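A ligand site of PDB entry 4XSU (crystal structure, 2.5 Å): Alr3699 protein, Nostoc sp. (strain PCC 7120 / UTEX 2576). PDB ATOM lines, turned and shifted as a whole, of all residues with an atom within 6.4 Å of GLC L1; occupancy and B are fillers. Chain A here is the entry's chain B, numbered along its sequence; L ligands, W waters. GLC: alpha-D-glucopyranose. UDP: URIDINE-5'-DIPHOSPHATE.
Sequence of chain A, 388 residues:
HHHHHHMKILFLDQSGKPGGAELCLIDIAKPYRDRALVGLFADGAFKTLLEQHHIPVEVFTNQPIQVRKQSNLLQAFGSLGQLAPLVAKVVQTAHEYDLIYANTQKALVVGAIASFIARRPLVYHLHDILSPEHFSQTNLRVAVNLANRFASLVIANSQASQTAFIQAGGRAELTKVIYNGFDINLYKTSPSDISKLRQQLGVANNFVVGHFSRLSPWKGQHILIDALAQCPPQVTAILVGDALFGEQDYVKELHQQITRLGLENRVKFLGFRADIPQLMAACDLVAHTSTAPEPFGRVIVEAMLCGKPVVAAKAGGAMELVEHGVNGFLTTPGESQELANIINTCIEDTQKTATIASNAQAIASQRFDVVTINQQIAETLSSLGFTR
An oxygen (O6) of GLC L1 lies within hydrogen-bond range of the side-chain amide nitrogen (ND2) of Asn 157 (3.1 Å). OE2 of Glu 294 is in hydrogen-bond range of O3 of GLC L1, 2.5 Å away. An oxygen (O3B) of UDP L2 is in salt-bridge range of the side-chain amino group (NZ) of Lys 219, at 2.8 Å. N of Gly 20 sits close to O2B of UDP L2, at 3.4 Å. ND1 of His 127 is in hydrogen-bond range of O6 of GLC L1, 2.8 Å away. The guanidinium group (NE) of Arg 298 lies close to an oxygen (O3') of UDP L2 (3.2 Å). N of Gly 297 is in hydrogen-bond range of O4 of GLC L1, at 3.0 Å. NH1 of Arg 214 lies within salt-bridge range of O1B of UDP L2, at 2.5 Å. N of Arg 298 is in hydrogen-bond range of O2A of UDP L2, at 3.3 Å. An oxygen (O3) of GLC L1 lies within hydrogen-bond range of the backbone NH (N) of Phe 296 (2.9 Å). The side-chain amide nitrogen of Asn 180 is in hydrogen-bond range of an oxygen (O6) of GLC L1 (3.2 Å).
O3B of UDP L2 is in hydrogen-bond range of O2 of GLC L1 (2.7 Å).
O of His 127 lies within hydrogen-bond range of ND2 of Asn 157 (3.3 Å). OD1 of Asn 180 lies within hydrogen-bond range of SG of Cys 24. The side-chain amide oxygen (OD1) of Asn 180 lies within hydrogen-bond range of the guanidinium group (NH1) of Arg 298. N of Asn 157 sits at hydrogen-bond distance from O of Leu 126. The side-chain carboxylate (OE2) of Glu 294 lies within salt-bridge range of the side-chain amino group (NZ) of Lys 219 (2.9 Å).
Merely in contact with GLC L1: Gly 20 (3.7 Å), Ala 21 (3.8 Å), Pro 295 (3.6 Å) and Arg 298 (3.6 Å). Hydrophobic or aromatic side chains that line GLC L1: His 127, Pro 295 and Phe 296. Within 4 Å of GLC L1: Gly 20, Ala 21, His 127, Asn 157, Asn 180, Glu 294, Pro 295, Phe 296, Gly 297 and Arg 298. Along chain A the residues within 4 Å of GLC L1 span positions 20 to 298. The nearest printed residue that does not touch GLC L1 is Asp 128 (4.1 Å).
Water W1 lies within hydrogen-bond range of an oxygen (O1) of GLC L1 (2.5 Å), the backbone NH of Ala 21 (2.6 Å), the backbone NH of Gly 20 (3.0 Å) and an oxygen (O2B) of UDP L2 (3.2 Å). Water W2 lies within hydrogen-bond range of O2 of GLC L1 (2.8 Å) and OD1 of Asp 128 (3.5 Å).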
ATOM      1  N   GLY A  19     -27.858  -4.535   8.988  1.00  0.00           N
ATOM      2  CA  GLY A  19     -27.288  -3.242   9.292  1.00  0.00           C
ATOM      3  C   GLY A  19     -28.090  -2.166   8.577  1.00  0.00           C
ATOM      4  O   GLY A  19     -29.107  -2.442   7.873  1.00  0.00           O
ATOM      5  N   GLY A  20     -27.638  -0.939   8.753  1.00  0.00           N
ATOM      6  CA  GLY A  20     -28.285   0.214   8.129  1.00  0.00           C
ATOM      7  C   GLY A  20     -28.431   0.113   6.629  1.00  0.00           C
ATOM      8  O   GLY A  20     -29.514   0.356   6.081  1.00  0.00           O
ATOM      9  N   ALA A  21     -27.347  -0.254   5.940  1.00  0.00           N
ATOM     10  CA  ALA A  21     -27.383  -0.301   4.478  1.00  0.00           C
ATOM     11  C   ALA A  21     -28.365  -1.354   4.062  1.00  0.00           C
ATOM     12  O   ALA A  21     -29.132  -1.174   3.124  1.00  0.00           O
ATOM     13  CB  ALA A  21     -26.025  -0.599   3.911  1.00  0.00           C
ATOM     14  N   GLU A  22     -28.375  -2.437   4.813  1.00  0.00           N
ATOM     15  CA  GLU A  22     -29.219  -3.586   4.502  1.00  0.00           C
ATOM     16  C   GLU A  22     -30.690  -3.265   4.733  1.00  0.00           C
ATOM     17  O   GLU A  22     -31.523  -3.539   3.874  1.00  0.00           O
ATOM     18  CB  GLU A  22     -28.771  -4.788   5.324  1.00  0.00           C
ATOM     19  CG  GLU A  22     -27.456  -5.380   4.825  1.00  0.00           C
ATOM     20  CD  GLU A  22     -26.240  -4.621   5.269  1.00  0.00           C
ATOM     21  OE1 GLU A  22     -26.321  -4.010   6.345  1.00  0.00           O
ATOM     22  OE2 GLU A  22     -25.192  -4.646   4.570  1.00  0.00           O
ATOM     23  N   CYS A  24     -31.895  -0.323   4.642  1.00  0.00           N
ATOM     24  CA  CYS A  24     -32.209   0.603   3.537  1.00  0.00           C
ATOM     25  C   CYS A  24     -32.590  -0.135   2.281  1.00  0.00           C
ATOM     26  O   CYS A  24     -33.494   0.284   1.551  1.00  0.00           O
ATOM     27  CB  CYS A  24     -31.071   1.576   3.274  1.00  0.00           C
ATOM     28  SG  CYS A  24     -31.504   2.890   2.108  1.00  0.00           S
ATOM     29  N   HIS A 125     -24.788   1.773  -5.065  1.00  0.00           N
ATOM     30  CA  HIS A 125     -25.380   2.527  -3.973  1.00  0.00           C
ATOM     31  C   HIS A 125     -24.387   2.689  -2.853  1.00  0.00           C
ATOM     32  O   HIS A 125     -24.079   1.734  -2.136  1.00  0.00           O
ATOM     33  CB  HIS A 125     -26.655   1.864  -3.464  1.00  0.00           C
ATOM     34  CG  HIS A 125     -27.598   2.830  -2.790  1.00  0.00           C
ATOM     35  ND1 HIS A 125     -28.924   2.956  -3.145  1.00  0.00           N
ATOM     36  CD2 HIS A 125     -27.383   3.718  -1.783  1.00  0.00           C
ATOM     37  CE1 HIS A 125     -29.496   3.865  -2.390  1.00  0.00           C
ATOM     38  NE2 HIS A 125     -28.577   4.353  -1.559  1.00  0.00           N
ATOM     39  N   LEU A 126     -23.918   3.918  -2.673  1.00  0.00           N
ATOM     40  CA  LEU A 126     -22.891   4.248  -1.725  1.00  0.00           C
ATOM     41  C   LEU A 126     -23.503   4.659  -0.371  1.00  0.00           C
ATOM     42  O   LEU A 126     -24.152   5.702  -0.284  1.00  0.00           O
ATOM     43  CB  LEU A 126     -22.062   5.404  -2.286  1.00  0.00           C
ATOM     44  CG  LEU A 126     -21.008   5.960  -1.347  1.00  0.00           C
ATOM     45  CD1 LEU A 126     -19.955   4.916  -1.028  1.00  0.00           C
ATOM     46  CD2 LEU A 126     -20.374   7.202  -1.966  1.00  0.00           C
ATOM     47  N   HIS A 127     -23.288   3.843   0.681  1.00  0.00           N
ATOM     48  CA  HIS A 127     -23.797   4.137   2.017  1.00  0.00           C
ATOM     49  C   HIS A 127     -22.677   4.494   2.961  1.00  0.00           C
ATOM     50  O   HIS A 127     -22.907   4.643   4.143  1.00  0.00           O
ATOM     51  CB  HIS A 127     -24.535   2.942   2.617  1.00  0.00           C
ATOM     52  CG  HIS A 127     -25.738   2.514   1.844  1.00  0.00           C
ATOM     53  ND1 HIS A 127     -26.966   3.119   1.999  1.00  0.00           N
ATOM     54  CD2 HIS A 127     -25.917   1.531   0.947  1.00  0.00           C
ATOM     55  CE1 HIS A 127     -27.841   2.516   1.224  1.00  0.00           C
ATOM     56  NE2 HIS A 127     -27.235   1.547   0.563  1.00  0.00           N
ATOM     57  N   ASP A 128     -21.457   4.601   2.457  1.00  0.00           N
ATOM     58  CA  ASP A 128     -20.321   4.899   3.335  1.00  0.00           C
ATOM     59  C   ASP A 128     -19.739   6.254   2.992  1.00  0.00           C
ATOM     60  O   ASP A 128     -20.008   6.823   1.945  1.00  0.00           O
ATOM     61  CB  ASP A 128     -19.207   3.842   3.204  1.00  0.00           C
ATOM     62  CG  ASP A 128     -19.713   2.384   3.296  1.00  0.00           C
ATOM     63  OD1 ASP A 128     -20.418   2.043   4.271  1.00  0.00           O
ATOM     64  OD2 ASP A 128     -19.349   1.575   2.403  1.00  0.00           O
ATOM     65  N   ASN A 157     -25.986   8.316  -0.259  1.00  0.00           N
ATOM     66  CA  ASN A 157     -27.050   8.446   0.719  1.00  0.00           C
ATOM     67  C   ASN A 157     -26.975   9.833   1.371  1.00  0.00           C
ATOM     68  O   ASN A 157     -27.734  10.140   2.264  1.00  0.00           O
ATOM     69  CB  ASN A 157     -26.926   7.336   1.761  1.00  0.00           C
ATOM     70  CG  ASN A 157     -25.603   7.380   2.460  1.00  0.00           C
ATOM     71  OD1 ASN A 157     -24.695   8.083   2.022  1.00  0.00           O
ATOM     72  ND2 ASN A 157     -25.470   6.625   3.553  1.00  0.00           N
ATOM     73  N   ASN A 180     -32.135   8.084   2.438  1.00  0.00           N
ATOM     74  CA  ASN A 180     -32.895   6.882   2.878  1.00  0.00           C
ATOM     75  C   ASN A 180     -34.361   7.241   3.013  1.00  0.00           C
ATOM     76  O   ASN A 180     -34.696   8.374   3.376  1.00  0.00           O
ATOM     77  CB  ASN A 180     -32.435   6.348   4.247  1.00  0.00           C
ATOM     78  CG  ASN A 180     -31.149   5.508   4.205  1.00  0.00           C
ATOM     79  OD1 ASN A 180     -31.017   4.539   4.947  1.00  0.00           O
ATOM     80  ND2 ASN A 180     -30.178   5.902   3.398  1.00  0.00           N
ATOM     81  N   ARG A 214     -25.366   0.114  16.835  1.00  0.00           N
ATOM     82  CA  ARG A 214     -24.501  -1.023  17.087  1.00  0.00           C
ATOM     83  C   ARG A 214     -23.312  -0.560  17.931  1.00  0.00           C
ATOM     84  O   ARG A 214     -22.916   0.594  17.892  1.00  0.00           O
ATOM     85  CB  ARG A 214     -24.053  -1.660  15.774  1.00  0.00           C
ATOM     86  CG  ARG A 214     -23.047  -0.836  14.987  1.00  0.00           C
ATOM     87  CD  ARG A 214     -22.968  -1.282  13.529  1.00  0.00           C
ATOM     88  NE  ARG A 214     -21.745  -0.779  12.919  1.00  0.00           N
ATOM     89  CZ  ARG A 214     -21.683   0.185  12.004  1.00  0.00           C
ATOM     90  NH1 ARG A 214     -22.767   0.756  11.563  1.00  0.00           N
ATOM     91  NH2 ARG A 214     -20.501   0.557  11.521  1.00  0.00           N
ATOM     92  N   TRP A 218     -16.716   3.920  17.316  1.00  0.00           N
ATOM     93  CA  TRP A 218     -17.001   5.100  16.524  1.00  0.00           C
ATOM     94  C   TRP A 218     -18.457   5.532  16.626  1.00  0.00           C
ATOM     95  O   TRP A 218     -18.787   6.655  16.227  1.00  0.00           O
ATOM     96  CB  TRP A 218     -16.528   4.946  15.055  1.00  0.00           C
ATOM     97  CG  TRP A 218     -17.474   4.271  14.106  1.00  0.00           C
ATOM     98  CD1 TRP A 218     -17.539   2.933  13.833  1.00  0.00           C
ATOM     99  CD2 TRP A 218     -18.457   4.901  13.256  1.00  0.00           C
ATOM    100  NE1 TRP A 218     -18.525   2.684  12.894  1.00  0.00           N
ATOM    101  CE2 TRP A 218     -19.097   3.878  12.525  1.00  0.00           C
ATOM    102  CE3 TRP A 218     -18.885   6.230  13.074  1.00  0.00           C
ATOM    103  CZ2 TRP A 218     -20.143   4.137  11.613  1.00  0.00           C
ATOM    104  CZ3 TRP A 218     -19.919   6.483  12.166  1.00  0.00           C
ATOM    105  CH2 TRP A 218     -20.537   5.437  11.453  1.00  0.00           C
ATOM    106  N   LYS A 219     -19.325   4.661  17.144  1.00  0.00           N
ATOM    107  CA  LYS A 219     -20.700   5.057  17.436  1.00  0.00           C
ATOM    108  C   LYS A 219     -20.836   5.851  18.760  1.00  0.00           C
ATOM    109  O   LYS A 219     -21.884   6.406  19.043  1.00  0.00           O
ATOM    110  CB  LYS A 219     -21.630   3.846  17.412  1.00  0.00           C
ATOM    111  CG  LYS A 219     -21.771   3.207  16.041  1.00  0.00           C
ATOM    112  CD  LYS A 219     -22.341   4.168  15.021  1.00  0.00           C
ATOM    113  CE  LYS A 219     -22.981   3.424  13.887  1.00  0.00           C
ATOM    114  NZ  LYS A 219     -23.479   4.330  12.821  1.00  0.00           N
ATOM    115  N   GLU A 294     -20.923  10.549  10.282  1.00  0.00           N
ATOM    116  CA  GLU A 294     -21.956   9.609   9.926  1.00  0.00           C
ATOM    117  C   GLU A 294     -22.377   9.783   8.482  1.00  0.00           C
ATOM    118  O   GLU A 294     -22.741  10.866   8.046  1.00  0.00           O
ATOM    119  CB  GLU A 294     -23.197   9.812  10.824  1.00  0.00           C
ATOM    120  CG  GLU A 294     -24.305   8.754  10.681  1.00  0.00           C
ATOM    121  CD  GLU A 294     -23.967   7.460  11.412  1.00  0.00           C
ATOM    122  OE1 GLU A 294     -23.467   7.571  12.575  1.00  0.00           O
ATOM    123  OE2 GLU A 294     -24.181   6.351  10.819  1.00  0.00           O
ATOM    124  N   PRO A 295     -22.364   8.697   7.719  1.00  0.00           N
ATOM    125  CA  PRO A 295     -22.814   8.835   6.371  1.00  0.00           C
ATOM    126  C   PRO A 295     -24.207   9.369   6.238  1.00  0.00           C
ATOM    127  O   PRO A 295     -24.425  10.269   5.444  1.00  0.00           O
ATOM    128  CB  PRO A 295     -22.739   7.416   5.844  1.00  0.00           C
ATOM    129  CG  PRO A 295     -21.494   6.903   6.515  1.00  0.00           C
ATOM    130  CD  PRO A 295     -21.560   7.476   7.892  1.00  0.00           C
ATOM    131  N   PHE A 296     -25.135   8.798   6.987  1.00  0.00           N
ATOM    132  CA  PHE A 296     -26.509   9.259   6.999  1.00  0.00           C
ATOM    133  C   PHE A 296     -27.028   9.299   8.442  1.00  0.00           C
ATOM    134  O   PHE A 296     -27.119  10.372   9.003  1.00  0.00           O
ATOM    135  CB  PHE A 296     -27.352   8.413   6.110  1.00  0.00           C
ATOM    136  CG  PHE A 296     -28.785   8.801   6.055  1.00  0.00           C
ATOM    137  CD1 PHE A 296     -29.205   9.862   5.268  1.00  0.00           C
ATOM    138  CD2 PHE A 296     -29.736   8.067   6.756  1.00  0.00           C
ATOM    139  CE1 PHE A 296     -30.551  10.187   5.180  1.00  0.00           C
ATOM    140  CE2 PHE A 296     -31.091   8.385   6.660  1.00  0.00           C
ATOM    141  CZ  PHE A 296     -31.499   9.440   5.877  1.00  0.00           C
ATOM    142  N   GLY A 297     -27.288   8.155   9.062  1.00  0.00           N
ATOM    143  CA  GLY A 297     -27.801   8.107  10.449  1.00  0.00           C
ATOM    144  C   GLY A 297     -29.298   7.867  10.457  1.00  0.00           C
ATOM    145  O   GLY A 297     -30.079   8.763  10.688  1.00  0.00           O
ATOM    146  N   ARG A 298     -29.709   6.655  10.140  1.00  0.00           N
ATOM    147  CA  ARG A 298     -31.101   6.339  10.070  1.00  0.00           C
ATOM    148  C   ARG A 298     -31.844   6.604  11.398  1.00  0.00           C
ATOM    149  O   ARG A 298     -33.032   6.913  11.412  1.00  0.00           O
ATOM    150  CB  ARG A 298     -31.259   4.876   9.701  1.00  0.00           C
ATOM    151  CG  ARG A 298     -31.038   4.569   8.251  1.00  0.00           C
ATOM    152  CD  ARG A 298     -30.948   3.066   8.049  1.00  0.00           C
ATOM    153  NE  ARG A 298     -32.251   2.422   8.192  1.00  0.00           N
ATOM    154  CZ  ARG A 298     -33.188   2.376   7.263  1.00  0.00           C
ATOM    155  NH1 ARG A 298     -33.025   2.921   6.062  1.00  0.00           N
ATOM    156  NH2 ARG A 298     -34.326   1.772   7.528  1.00  0.00           N
ATOM    157  N   VAL A 299     -31.153   6.420  12.519  1.00  0.00           N
ATOM    158  CA  VAL A 299     -31.795   6.556  13.816  1.00  0.00           C
ATOM    159  C   VAL A 299     -32.233   7.996  14.092  1.00  0.00           C
ATOM    160  O   VAL A 299     -33.238   8.214  14.778  1.00  0.00           O
ATOM    161  CB  VAL A 299     -30.900   6.061  14.951  1.00  0.00           C
ATOM    162  CG1 VAL A 299     -30.743   4.561  14.876  1.00  0.00           C
ATOM    163  CG2 VAL A 299     -29.529   6.719  14.949  1.00  0.00           C
HETATM  164  C1  GLC L   1     -24.313   3.221   6.289  1.00  0.00           C
HETATM  165  C2  GLC L   1     -23.995   4.261   7.359  1.00  0.00           C
HETATM  166  C3  GLC L   1     -25.230   4.917   7.968  1.00  0.00           C
HETATM  167  C4  GLC L   1     -26.319   4.998   6.925  1.00  0.00           C
HETATM  168  C5  GLC L   1     -26.764   3.619   6.565  1.00  0.00           C
HETATM  169  C6  GLC L   1     -27.936   3.715   5.564  1.00  0.00           C
HETATM  170  O1  GLC L   1     -23.776   1.955   6.671  1.00  0.00           O
HETATM  171  O2  GLC L   1     -23.028   3.772   8.303  1.00  0.00           O
HETATM  172  O3  GLC L   1     -24.970   6.257   8.431  1.00  0.00           O
HETATM  173  O4  GLC L   1     -27.487   5.556   7.481  1.00  0.00           O
HETATM  174  O5  GLC L   1     -25.687   3.150   5.834  1.00  0.00           O
HETATM  175  O6  GLC L   1     -27.538   4.462   4.397  1.00  0.00           O
HETATM  176  N1  UDP L   2     -31.528  -0.896  14.363  1.00  0.00           N
HETATM  177  C2  UDP L   2     -32.211  -1.986  14.926  1.00  0.00           C
HETATM  178  N3  UDP L   2     -31.863  -2.466  16.123  1.00  0.00           N
HETATM  179  C4  UDP L   2     -30.851  -1.911  16.800  1.00  0.00           C
HETATM  180  C5  UDP L   2     -30.164  -0.833  16.278  1.00  0.00           C
HETATM  181  C6  UDP L   2     -30.516  -0.331  15.031  1.00  0.00           C
HETATM  182  O2  UDP L   2     -33.153  -2.520  14.299  1.00  0.00           O
HETATM  183  O4  UDP L   2     -30.532  -2.367  17.926  1.00  0.00           O
HETATM  184  C1' UDP L   2     -31.914  -0.378  13.045  1.00  0.00           C
HETATM  185  C2' UDP L   2     -32.480   1.024  13.193  1.00  0.00           C
HETATM  186  O2' UDP L   2     -33.824   1.072  12.693  1.00  0.00           O
HETATM  187  C3' UDP L   2     -31.586   1.934  12.377  1.00  0.00           C
HETATM  188  C4' UDP L   2     -30.523   1.041  11.764  1.00  0.00           C
HETATM  189  O4' UDP L   2     -30.768  -0.306  12.196  1.00  0.00           O
HETATM  190  O3' UDP L   2     -32.349   2.567  11.344  1.00  0.00           O
HETATM  191  C5' UDP L   2     -29.125   1.478  12.197  1.00  0.00           C
HETATM  192  O5' UDP L   2     -28.474   2.143  11.116  1.00  0.00           O
HETATM  193  PA  UDP L   2     -27.622   3.481  11.385  1.00  0.00           P
HETATM  194  O1A UDP L   2     -28.187   4.168  12.608  1.00  0.00           O
HETATM  195  O2A UDP L   2     -27.516   4.237  10.076  1.00  0.00           O
HETATM  196  O3A UDP L   2     -26.168   2.902  11.749  1.00  0.00           O
HETATM  197  PB  UDP L   2     -25.350   2.009  10.689  1.00  0.00           P
HETATM  198  O1B UDP L   2     -25.259   0.657  11.355  1.00  0.00           O
HETATM  199  O2B UDP L   2     -26.204   2.049   9.445  1.00  0.00           O
HETATM  200  O3B UDP L   2     -24.023   2.732  10.551  1.00  0.00           O
HETATM  201  O   HOH W   1     -25.184  -0.064   7.331  1.00  0.00           O
HETATM  202  O   HOH W   2     -20.378   3.392   7.495  1.00  0.00           O
